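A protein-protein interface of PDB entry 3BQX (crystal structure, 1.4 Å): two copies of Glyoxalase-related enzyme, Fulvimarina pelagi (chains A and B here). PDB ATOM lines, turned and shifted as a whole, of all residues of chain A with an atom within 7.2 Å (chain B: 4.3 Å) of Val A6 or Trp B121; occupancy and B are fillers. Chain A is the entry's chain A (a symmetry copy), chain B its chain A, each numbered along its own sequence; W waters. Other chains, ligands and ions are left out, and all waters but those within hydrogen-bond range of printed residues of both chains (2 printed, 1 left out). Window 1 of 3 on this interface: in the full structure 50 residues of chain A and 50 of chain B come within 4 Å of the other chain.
Val A6 touches just these residues of chain B: Met B43 (3.8 Å), Asn B44 (2.9 Å), Phe B46 (3.3 Å), Ala B74 (3.4 Å) and Trp B121 (3.7 Å).
Of chain A, only Val A6 (3.7 Å) comes within 4 Å of Trp B121.
Printed residues of chain A within 4 Å of Met B43: Gln A4 (3.6 Å), Gln A5 (3.5 Å) and Val A6 (3.8 Å).
Of the printed residues of chain A, Phe B46 touches Val A6 (3.3 Å).
Printed residues of chain A within 4 Å of Ala B74: Val A6 (3.4 Å), Ala A7 (2.7 Å) and Val A8 (2.9 Å).
Of the printed residues of chain A, Trp B29 touches Leu A3, Gln A4 and Gln A5.
Of the printed residues of chain B, Gln A5 touches Trp B29 (3.9 Å), Met B43 (3.5 Å) and Asn B44 (3.2 Å).
The nearest printed residue of chain B that does not touch Val A6 is Ile B9 (4.3 Å).
The nearest printed residue of chain A that does not touch Met B43 is Leu A3 (5.7 Å).
Among the printed residues, merely in contact across the chains: Gln A4 with Trp B29 (3.3 Å), Gln A4 with Met B43 (3.6 Å), Gln A5 with Trp B29 (3.9 Å), Gln A5 with Met B43 (3.5 Å), Gln A5 with Asn B44 (3.2 Å), Val A6 with Met B43 (3.8 Å), Val A6 with Phe B46 (3.3 Å), Val A6 with Ala B74 (3.4 Å), Val A6 with Trp B121 (3.7 Å), Val A8 with Leu B73 (3.5 Å) and Ile A9 with Ile B9 (3.5 Å).
Of the 11 printed residues of chain A, 8 touch a printed residue of chain B.
Hydrophobic or aromatic side chains of chain A within 4 Å of the printed part of chain B: Val A6, Ala A7, Val A8 and Ile A9.
Hydrophobic or aromatic side chains of chain B within 4 Å of the printed part of chain A: Ile B9, Trp B29, Met B43, Phe B46, Ala B74 and Trp B121.
The backbone carbonyl oxygen (O) of Tyr B23 sits at hydrogen-bond distance from the backbone NH (N) of Trp B29 (2.9 Å).
The side-chain hydroxyl (OH) of Tyr B23 is in hydrogen-bond range of the indole nitrogen (NE1) of Trp B121 (2.9 Å).
O of Ile B120 lies within hydrogen-bond range of N of Leu B73 (2.9 Å).
N of Trp B121 lies within hydrogen-bond range of O of Val B113, at 2.9 Å.
The backbone carbonyl oxygen (O) of Ala A7 is in hydrogen-bond range of the backbone NH (N) of Val A47 (3.0 Å).
The backbone NH of Ile A9 is in hydrogen-bond range of the backbone carbonyl oxygen of Val A47 (2.9 Å).
The indole nitrogen (NE1) of Trp B29 is in hydrogen-bond range of the backbone carbonyl oxygen (O) of Leu A3, at 3.0 Å.
The backbone NH (N) of Asn B44 is in hydrogen-bond range of the backbone carbonyl oxygen (O) of Gln A4.
The side-chain amide oxygen (OD1) of Asn B44 lies within hydrogen-bond range of the backbone NH (N) of Val A6 (2.9 Å).
ND2 of Asn B44 is in hydrogen-bond range of O of Gly A45 (2.8 Å).
O of Ala B74 sits at hydrogen-bond distance from N of Ala A7.
The backbone NH of Ala B74 sits at hydrogen-bond distance from the backbone carbonyl oxygen of Val A8, at 2.9 Å.
Ile A9 touches its own counterpart, Ile B9.
Positions printed for both chains: 9 and 46.
Water W1 lies within hydrogen-bond range of OG1 of Thr A10 (2.6 Å), O of Val A8 (3.3 Å) and N of Ala B74 (3.5 Å).
Water W2 lies within hydrogen-bond range of O of Phe B27 (3.2 Å) and N of Leu A3 (3.3 Å).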
ATOM      1  N   LEU A   3      24.903  31.342   2.277  1.00  0.00           N
ATOM      2  CA  LEU A   3      23.422  31.188   2.370  1.00  0.00           C
ATOM      3  C   LEU A   3      23.000  29.765   2.709  1.00  0.00           C
ATOM      4  O   LEU A   3      23.676  28.797   2.359  1.00  0.00           O
ATOM      5  CB  LEU A   3      22.750  31.617   1.062  1.00  0.00           C
ATOM      6  CG  LEU A   3      22.438  33.105   0.895  1.00  0.00           C
ATOM      7  CD1 LEU A   3      23.728  33.900   0.799  1.00  0.00           C
ATOM      8  CD2 LEU A   3      21.589  33.303  -0.353  1.00  0.00           C
ATOM      9  N   GLN A   4      21.864  29.650   3.383  1.00  0.00           N
ATOM     10  CA  GLN A   4      21.338  28.354   3.791  1.00  0.00           C
ATOM     11  C   GLN A   4      20.669  27.664   2.610  1.00  0.00           C
ATOM     12  O   GLN A   4      19.458  27.763   2.394  1.00  0.00           O
ATOM     13  CB  GLN A   4      20.388  28.565   4.971  1.00  0.00           C
ATOM     14  CG  GLN A   4      21.151  29.158   6.148  1.00  0.00           C
ATOM     15  CD  GLN A   4      20.323  29.373   7.392  1.00  0.00           C
ATOM     16  OE1 GLN A   4      19.233  28.812   7.550  1.00  0.00           O
ATOM     17  NE2 GLN A   4      20.854  30.174   8.304  1.00  0.00           N
ATOM     18  N   GLN A   5      21.489  26.927   1.865  1.00  0.00           N
ATOM     19  CA  GLN A   5      21.042  26.261   0.657  1.00  0.00           C
ATOM     20  C   GLN A   5      21.609  24.871   0.396  1.00  0.00           C
ATOM     21  O   GLN A   5      22.774  24.588   0.673  1.00  0.00           O
ATOM     22  CB  GLN A   5      21.385  27.155  -0.546  1.00  0.00           C
ATOM     23  CG  GLN A   5      21.154  26.537  -1.926  1.00  0.00           C
ATOM     24  CD  GLN A   5      22.437  26.430  -2.748  1.00  0.00           C
ATOM     25  OE1 GLN A   5      23.229  25.500  -2.582  1.00  0.00           O
ATOM     26  NE2 GLN A   5      22.649  27.396  -3.634  1.00  0.00           N
ATOM     27  N   VAL A   6      20.750  24.010  -0.133  1.00  0.00           N
ATOM     28  CA  VAL A   6      21.137  22.671  -0.558  1.00  0.00           C
ATOM     29  C   VAL A   6      20.711  22.732  -2.010  1.00  0.00           C
ATOM     30  O   VAL A   6      19.553  23.025  -2.297  1.00  0.00           O
ATOM     31  CB  VAL A   6      20.363  21.552   0.166  1.00  0.00           C
ATOM     32  CG1 VAL A   6      20.548  20.225  -0.578  1.00  0.00           C
ATOM     33  CG2 VAL A   6      20.882  21.410   1.589  1.00  0.00           C
ATOM     34  N   ALA A   7      21.648  22.492  -2.922  1.00  0.00           N
ATOM     35  CA  ALA A   7      21.380  22.544  -4.352  1.00  0.00           C
ATOM     36  C   ALA A   7      20.932  21.199  -4.913  1.00  0.00           C
ATOM     37  O   ALA A   7      20.098  21.132  -5.818  1.00  0.00           O
ATOM     38  CB  ALA A   7      22.632  23.014  -5.093  1.00  0.00           C
ATOM     39  N   VAL A   8      21.502  20.124  -4.380  1.00  0.00           N
ATOM     40  CA  VAL A   8      21.177  18.783  -4.851  1.00  0.00           C
ATOM     41  C   VAL A   8      21.244  17.772  -3.728  1.00  0.00           C
ATOM     42  O   VAL A   8      22.136  17.848  -2.884  1.00  0.00           O
ATOM     43  CB  VAL A   8      22.196  18.288  -5.916  1.00  0.00           C
ATOM     44  CG1 VAL A   8      21.746  16.963  -6.495  1.00  0.00           C
ATOM     45  CG2 VAL A   8      22.383  19.322  -7.004  1.00  0.00           C
ATOM     46  N   ILE A   9      20.284  16.851  -3.706  1.00  0.00           N
ATOM     47  CA  ILE A   9      20.289  15.746  -2.752  1.00  0.00           C
ATOM     48  C   ILE A   9      20.604  14.580  -3.678  1.00  0.00           C
ATOM     49  O   ILE A   9      19.834  14.292  -4.592  1.00  0.00           O
ATOM     50  CB  ILE A   9      18.910  15.441  -2.120  1.00  0.00           C
ATOM     51  CG1 ILE A   9      18.437  16.617  -1.276  1.00  0.00           C
ATOM     52  CG2 ILE A   9      18.999  14.155  -1.280  1.00  0.00           C
ATOM     53  CD1 ILE A   9      17.047  16.415  -0.687  1.00  0.00           C
ATOM     54  N   THR A  10      21.738  13.929  -3.479  1.00  0.00           N
ATOM     55  CA  THR A  10      22.089  12.807  -4.337  1.00  0.00           C
ATOM     56  C   THR A  10      22.024  11.510  -3.563  1.00  0.00           C
ATOM     57  O   THR A  10      22.664  11.362  -2.524  1.00  0.00           O
ATOM     58  CB  THR A  10      23.507  12.958  -4.909  1.00  0.00           C
ATOM     59  OG1 THR A  10      23.562  14.125  -5.734  1.00  0.00           O
ATOM     60  CG2 THR A  10      23.883  11.751  -5.758  1.00  0.00           C
ATOM     61  N   GLY A  45      12.952  23.864  -4.932  1.00  0.00           N
ATOM     62  CA  GLY A  45      14.097  24.685  -4.584  1.00  0.00           C
ATOM     63  C   GLY A  45      15.441  24.025  -4.797  1.00  0.00           C
ATOM     64  O   GLY A  45      16.483  24.666  -4.660  1.00  0.00           O
ATOM     65  N   PHE A  46      15.420  22.744  -5.146  1.00  0.00           N
ATOM     66  CA  PHE A  46      16.648  21.981  -5.337  1.00  0.00           C
ATOM     67  C   PHE A  46      16.357  20.816  -6.269  1.00  0.00           C
ATOM     68  O   PHE A  46      15.215  20.605  -6.681  1.00  0.00           O
ATOM     69  CB  PHE A  46      17.123  21.446  -3.984  1.00  0.00           C
ATOM     70  CG  PHE A  46      16.222  20.386  -3.409  1.00  0.00           C
ATOM     71  CD1 PHE A  46      16.489  19.038  -3.633  1.00  0.00           C
ATOM     72  CD2 PHE A  46      15.077  20.738  -2.706  1.00  0.00           C
ATOM     73  CE1 PHE A  46      15.627  18.048  -3.165  1.00  0.00           C
ATOM     74  CE2 PHE A  46      14.204  19.751  -2.233  1.00  0.00           C
ATOM     75  CZ  PHE A  46      14.484  18.408  -2.468  1.00  0.00           C
ATOM     76  N   VAL A  47      17.398  20.054  -6.577  1.00  0.00           N
ATOM     77  CA  VAL A  47      17.294  18.898  -7.454  1.00  0.00           C
ATOM     78  C   VAL A  47      17.572  17.613  -6.682  1.00  0.00           C
ATOM     79  O   VAL A  47      18.469  17.579  -5.835  1.00  0.00           O
ATOM     80  CB  VAL A  47      18.321  19.011  -8.603  1.00  0.00           C
ATOM     81  CG1 VAL A  47      18.233  17.814  -9.526  1.00  0.00           C
ATOM     82  CG2 VAL A  47      18.083  20.295  -9.376  1.00  0.00           C
ATOM     83  N   ILE B   9      15.040  17.289   5.307  1.00  0.00           N
ATOM     84  CA  ILE B   9      16.164  16.378   5.106  1.00  0.00           C
ATOM     85  C   ILE B   9      16.616  16.174   6.545  1.00  0.00           C
ATOM     86  O   ILE B   9      17.012  17.129   7.210  1.00  0.00           O
ATOM     87  CB  ILE B   9      17.365  17.000   4.356  1.00  0.00           C
ATOM     88  CG1 ILE B   9      16.971  17.372   2.933  1.00  0.00           C
ATOM     89  CG2 ILE B   9      18.547  16.015   4.366  1.00  0.00           C
ATOM     90  CD1 ILE B   9      18.087  18.063   2.161  1.00  0.00           C
ATOM     91  N   PHE B  22      29.808  22.632  13.087  1.00  0.00           N
ATOM     92  CA  PHE B  22      30.023  22.462  11.657  1.00  0.00           C
ATOM     93  C   PHE B  22      29.077  23.331  10.832  1.00  0.00           C
ATOM     94  O   PHE B  22      29.509  24.087   9.965  1.00  0.00           O
ATOM     95  CB  PHE B  22      29.829  20.996  11.258  1.00  0.00           C
ATOM     96  CG  PHE B  22      30.040  20.732   9.790  1.00  0.00           C
ATOM     97  CD1 PHE B  22      31.326  20.677   9.256  1.00  0.00           C
ATOM     98  CD2 PHE B  22      28.953  20.541   8.936  1.00  0.00           C
ATOM     99  CE1 PHE B  22      31.529  20.435   7.896  1.00  0.00           C
ATOM    100  CE2 PHE B  22      29.148  20.299   7.572  1.00  0.00           C
ATOM    101  CZ  PHE B  22      30.438  20.246   7.053  1.00  0.00           C
ATOM    102  N   TYR B  23      27.779  23.232  11.105  1.00  0.00           N
ATOM    103  CA  TYR B  23      26.810  24.007  10.340  1.00  0.00           C
ATOM    104  C   TYR B  23      26.809  25.488  10.688  1.00  0.00           C
ATOM    105  O   TYR B  23      26.588  26.331   9.818  1.00  0.00           O
ATOM    106  CB  TYR B  23      25.410  23.384  10.491  1.00  0.00           C
ATOM    107  CG  TYR B  23      25.347  22.031   9.806  1.00  0.00           C
ATOM    108  CD1 TYR B  23      25.385  21.935   8.418  1.00  0.00           C
ATOM    109  CD2 TYR B  23      25.381  20.857  10.546  1.00  0.00           C
ATOM    110  CE1 TYR B  23      25.473  20.706   7.782  1.00  0.00           C
ATOM    111  CE2 TYR B  23      25.475  19.615   9.925  1.00  0.00           C
ATOM    112  CZ  TYR B  23      25.526  19.549   8.539  1.00  0.00           C
ATOM    113  OH  TYR B  23      25.678  18.330   7.918  1.00  0.00           O
ATOM    114  N   PHE B  27      29.441  26.421   7.879  1.00  0.00           N
ATOM    115  CA  PHE B  27      28.580  26.956   6.826  1.00  0.00           C
ATOM    116  C   PHE B  27      28.063  28.364   7.104  1.00  0.00           C
ATOM    117  O   PHE B  27      27.680  29.078   6.179  1.00  0.00           O
ATOM    118  CB  PHE B  27      27.373  26.038   6.596  1.00  0.00           C
ATOM    119  CG  PHE B  27      27.585  24.993   5.531  1.00  0.00           C
ATOM    120  CD1 PHE B  27      27.525  23.641   5.848  1.00  0.00           C
ATOM    121  CD2 PHE B  27      27.813  25.362   4.208  1.00  0.00           C
ATOM    122  CE1 PHE B  27      27.686  22.668   4.860  1.00  0.00           C
ATOM    123  CE2 PHE B  27      27.975  24.401   3.210  1.00  0.00           C
ATOM    124  CZ  PHE B  27      27.909  23.049   3.540  1.00  0.00           C
ATOM    125  N   TRP B  29      25.440  28.934   9.060  1.00  0.00           N
ATOM    126  CA  TRP B  29      23.989  28.835   9.169  1.00  0.00           C
ATOM    127  C   TRP B  29      23.512  28.971  10.608  1.00  0.00           C
ATOM    128  O   TRP B  29      24.224  28.629  11.552  1.00  0.00           O
ATOM    129  CB  TRP B  29      23.511  27.503   8.587  1.00  0.00           C
ATOM    130  CG  TRP B  29      23.914  27.309   7.159  1.00  0.00           C
ATOM    131  CD1 TRP B  29      24.338  28.272   6.290  1.00  0.00           C
ATOM    132  CD2 TRP B  29      23.899  26.080   6.415  1.00  0.00           C
ATOM    133  NE1 TRP B  29      24.585  27.727   5.053  1.00  0.00           N
ATOM    134  CE2 TRP B  29      24.326  26.382   5.103  1.00  0.00           C
ATOM    135  CE3 TRP B  29      23.566  24.755   6.731  1.00  0.00           C
ATOM    136  CZ2 TRP B  29      24.433  25.410   4.107  1.00  0.00           C
ATOM    137  CZ3 TRP B  29      23.673  23.783   5.732  1.00  0.00           C
ATOM    138  CH2 TRP B  29      24.104  24.120   4.440  1.00  0.00           C
ATOM    139  N   MET B  43      15.922  26.133   5.143  1.00  0.00           N
ATOM    140  CA  MET B  43      16.669  26.158   3.896  1.00  0.00           C
ATOM    141  C   MET B  43      15.860  26.726   2.730  1.00  0.00           C
ATOM    142  O   MET B  43      14.807  27.343   2.928  1.00  0.00           O
ATOM    143  CB  MET B  43      17.158  24.745   3.565  1.00  0.00           C
ATOM    144  CG  MET B  43      17.850  24.053   4.765  1.00  0.00           C
ATOM    145  SD  MET B  43      19.491  24.855   5.441  1.00  0.00           S
ATOM    146  CE  MET B  43      20.623  24.279   4.010  1.00  0.00           C
ATOM    147  N   ASN B  44      16.351  26.504   1.514  1.00  0.00           N
ATOM    148  CA  ASN B  44      15.726  27.000   0.288  1.00  0.00           C
ATOM    149  C   ASN B  44      14.547  26.156  -0.184  1.00  0.00           C
ATOM    150  O   ASN B  44      14.619  25.478  -1.208  1.00  0.00           O
ATOM    151  CB  ASN B  44      16.781  27.093  -0.825  1.00  0.00           C
ATOM    152  CG  ASN B  44      17.570  25.799  -0.997  1.00  0.00           C
ATOM    153  OD1 ASN B  44      18.090  25.254  -0.027  1.00  0.00           O
ATOM    154  ND2 ASN B  44      17.666  25.317  -2.227  1.00  0.00           N
ATOM    155  N   PHE B  46      12.852  23.992   2.032  1.00  0.00           N
ATOM    156  CA  PHE B  46      12.686  22.859   2.933  1.00  0.00           C
ATOM    157  C   PHE B  46      13.481  23.124   4.201  1.00  0.00           C
ATOM    158  O   PHE B  46      14.173  24.137   4.313  1.00  0.00           O
ATOM    159  CB  PHE B  46      13.218  21.594   2.253  1.00  0.00           C
ATOM    160  CG  PHE B  46      14.713  21.594   2.075  1.00  0.00           C
ATOM    161  CD1 PHE B  46      15.535  20.996   3.027  1.00  0.00           C
ATOM    162  CD2 PHE B  46      15.296  22.246   0.996  1.00  0.00           C
ATOM    163  CE1 PHE B  46      16.923  21.048   2.910  1.00  0.00           C
ATOM    164  CE2 PHE B  46      16.689  22.304   0.871  1.00  0.00           C
ATOM    165  CZ  PHE B  46      17.497  21.704   1.833  1.00  0.00           C
ATOM    166  N   LEU B  73      25.061  15.618  -0.163  1.00  0.00           N
ATOM    167  CA  LEU B  73      24.284  16.850  -0.285  1.00  0.00           C
ATOM    168  C   LEU B  73      25.202  17.893  -0.900  1.00  0.00           C
ATOM    169  O   LEU B  73      26.330  18.063  -0.456  1.00  0.00           O
ATOM    170  CB  LEU B  73      23.819  17.340   1.087  1.00  0.00           C
ATOM    171  CG  LEU B  73      22.948  16.351   1.858  1.00  0.00           C
ATOM    172  CD1 LEU B  73      22.594  16.938   3.204  1.00  0.00           C
ATOM    173  CD2 LEU B  73      21.689  16.035   1.061  1.00  0.00           C
ATOM    174  N   ALA B  74      24.729  18.611  -1.909  1.00  0.00           N
ATOM    175  CA  ALA B  74      25.563  19.616  -2.547  1.00  0.00           C
ATOM    176  C   ALA B  74      25.110  21.024  -2.206  1.00  0.00           C
ATOM    177  O   ALA B  74      23.913  21.285  -2.061  1.00  0.00           O
ATOM    178  CB  ALA B  74      25.544  19.420  -4.062  1.00  0.00           C
ATOM    179  N   GLY B 111      34.452  20.058  -4.733  1.00  0.00           N
ATOM    180  CA  GLY B 111      35.200  19.262  -3.780  1.00  0.00           C
ATOM    181  C   GLY B 111      34.229  18.629  -2.800  1.00  0.00           C
ATOM    182  O   GLY B 111      33.027  18.901  -2.858  1.00  0.00           O
ATOM    183  N   TYR B 112      34.729  17.789  -1.901  1.00  0.00           N
ATOM    184  CA  TYR B 112      33.874  17.127  -0.921  1.00  0.00           C
ATOM    185  C   TYR B 112      34.417  17.232   0.498  1.00  0.00           C
ATOM    186  O   TYR B 112      35.625  17.108   0.727  1.00  0.00           O
ATOM    187  CB  TYR B 112      33.706  15.646  -1.271  1.00  0.00           C
ATOM    188  CG  TYR B 112      32.813  15.357  -2.458  1.00  0.00           C
ATOM    189  CD1 TYR B 112      31.426  15.270  -2.309  1.00  0.00           C
ATOM    190  CD2 TYR B 112      33.355  15.115  -3.726  1.00  0.00           C
ATOM    191  CE1 TYR B 112      30.606  14.938  -3.385  1.00  0.00           C
ATOM    192  CE2 TYR B 112      32.541  14.788  -4.806  1.00  0.00           C
ATOM    193  CZ  TYR B 112      31.168  14.697  -4.626  1.00  0.00           C
ATOM    194  OH  TYR B 112      30.356  14.326  -5.675  1.00  0.00           O
ATOM    195  N   VAL B 113      33.516  17.462   1.449  1.00  0.00           N
ATOM    196  CA  VAL B 113      33.861  17.556   2.861  1.00  0.00           C
ATOM    197  C   VAL B 113      32.718  16.921   3.632  1.00  0.00           C
ATOM    198  O   VAL B 113      31.553  17.232   3.377  1.00  0.00           O
ATOM    199  CB  VAL B 113      34.011  19.028   3.321  1.00  0.00           C
ATOM    200  CG1 VAL B 113      34.279  19.079   4.819  1.00  0.00           C
ATOM    201  CG2 VAL B 113      35.141  19.705   2.559  1.00  0.00           C
ATOM    202  N   HIS B 119      28.372  12.625   7.144  1.00  0.00           N
ATOM    203  CA  HIS B 119      27.492  12.968   6.026  1.00  0.00           C
ATOM    204  C   HIS B 119      28.268  13.799   5.020  1.00  0.00           C
ATOM    205  O   HIS B 119      28.816  14.847   5.347  1.00  0.00           O
ATOM    206  CB  HIS B 119      26.268  13.722   6.529  1.00  0.00           C
ATOM    207  CG  HIS B 119      25.451  12.938   7.503  1.00  0.00           C
ATOM    208  ND1 HIS B 119      24.837  11.749   7.169  1.00  0.00           N
ATOM    209  CD2 HIS B 119      25.175  13.152   8.810  1.00  0.00           C
ATOM    210  CE1 HIS B 119      24.219  11.264   8.232  1.00  0.00           C
ATOM    211  NE2 HIS B 119      24.408  12.098   9.240  1.00  0.00           N
ATOM    212  N   ILE B 120      28.292  13.322   3.782  1.00  0.00           N
ATOM    213  CA  ILE B 120      29.033  13.963   2.710  1.00  0.00           C
ATOM    214  C   ILE B 120      28.421  15.207   2.084  1.00  0.00           C
ATOM    215  O   ILE B 120      27.255  15.212   1.671  1.00  0.00           O
ATOM    216  CB  ILE B 120      29.303  12.951   1.574  1.00  0.00           C
ATOM    217  CG1 ILE B 120      30.075  11.749   2.131  1.00  0.00           C
ATOM    218  CG2 ILE B 120      30.068  13.619   0.450  1.00  0.00           C
ATOM    219  CD1 ILE B 120      30.244  10.615   1.135  1.00  0.00           C
ATOM    220  N   TRP B 121      29.223  16.263   2.012  1.00  0.00           N
ATOM    221  CA  TRP B 121      28.797  17.503   1.395  1.00  0.00           C
ATOM    222  C   TRP B 121      29.667  17.809   0.194  1.00  0.00           C
ATOM    223  O   TRP B 121      30.896  17.700   0.260  1.00  0.00           O
ATOM    224  CB  TRP B 121      28.910  18.685   2.363  1.00  0.00           C
ATOM    225  CG  TRP B 121      27.789  18.791   3.321  1.00  0.00           C
ATOM    226  CD1 TRP B 121      27.703  18.209   4.549  1.00  0.00           C
ATOM    227  CD2 TRP B 121      26.558  19.491   3.116  1.00  0.00           C
ATOM    228  NE1 TRP B 121      26.486  18.498   5.129  1.00  0.00           N
ATOM    229  CE2 TRP B 121      25.768  19.286   4.269  1.00  0.00           C
ATOM    230  CE3 TRP B 121      26.045  20.274   2.072  1.00  0.00           C
ATOM    231  CZ2 TRP B 121      24.490  19.833   4.407  1.00  0.00           C
ATOM    232  CZ3 TRP B 121      24.764  20.818   2.214  1.00  0.00           C
ATOM    233  CH2 TRP B 121      24.009  20.594   3.372  1.00  0.00           C
ATOM    234  N   GLU B 122      29.038  18.170  -0.914  1.00  0.00           N
ATOM    235  CA  GLU B 122      29.777  18.571  -2.094  1.00  0.00           C
ATOM    236  C   GLU B 122      29.684  20.090  -2.131  1.00  0.00           C
ATOM    237  O   GLU B 122      28.598  20.644  -1.970  1.00  0.00           O
ATOM    238  CB  GLU B 122      29.152  18.014  -3.376  1.00  0.00           C
ATOM    239  CG  GLU B 122      29.785  18.609  -4.641  1.00  0.00           C
ATOM    240  CD  GLU B 122      29.154  18.096  -5.914  1.00  0.00           C
ATOM    241  OE1 GLU B 122      28.003  17.619  -5.851  1.00  0.00           O
ATOM    242  OE2 GLU B 122      29.802  18.187  -6.982  1.00  0.00           O
ATOM    243  N   ILE B 123      30.819  20.764  -2.288  1.00  0.00           N
ATOM    244  CA  ILE B 123      30.820  22.214  -2.406  1.00  0.00           C
ATOM    245  C   ILE B 123      31.152  22.391  -3.874  1.00  0.00           C
ATOM    246  O   ILE B 123      32.226  21.996  -4.329  1.00  0.00           O
ATOM    247  CB  ILE B 123      31.888  22.878  -1.521  1.00  0.00           C
ATOM    248  CG1 ILE B 123      31.670  22.474  -0.058  1.00  0.00           C
ATOM    249  CG2 ILE B 123      31.818  24.387  -1.676  1.00  0.00           C
ATOM    250  CD1 ILE B 123      30.276  22.764   0.477  1.00  0.00           C
HETATM  251  O   HOH W   1      24.595  16.068  -4.271  1.00  0.00           O
HETATM  252  O   HOH W   2      27.723  29.848   3.118  1.00  0.00           O
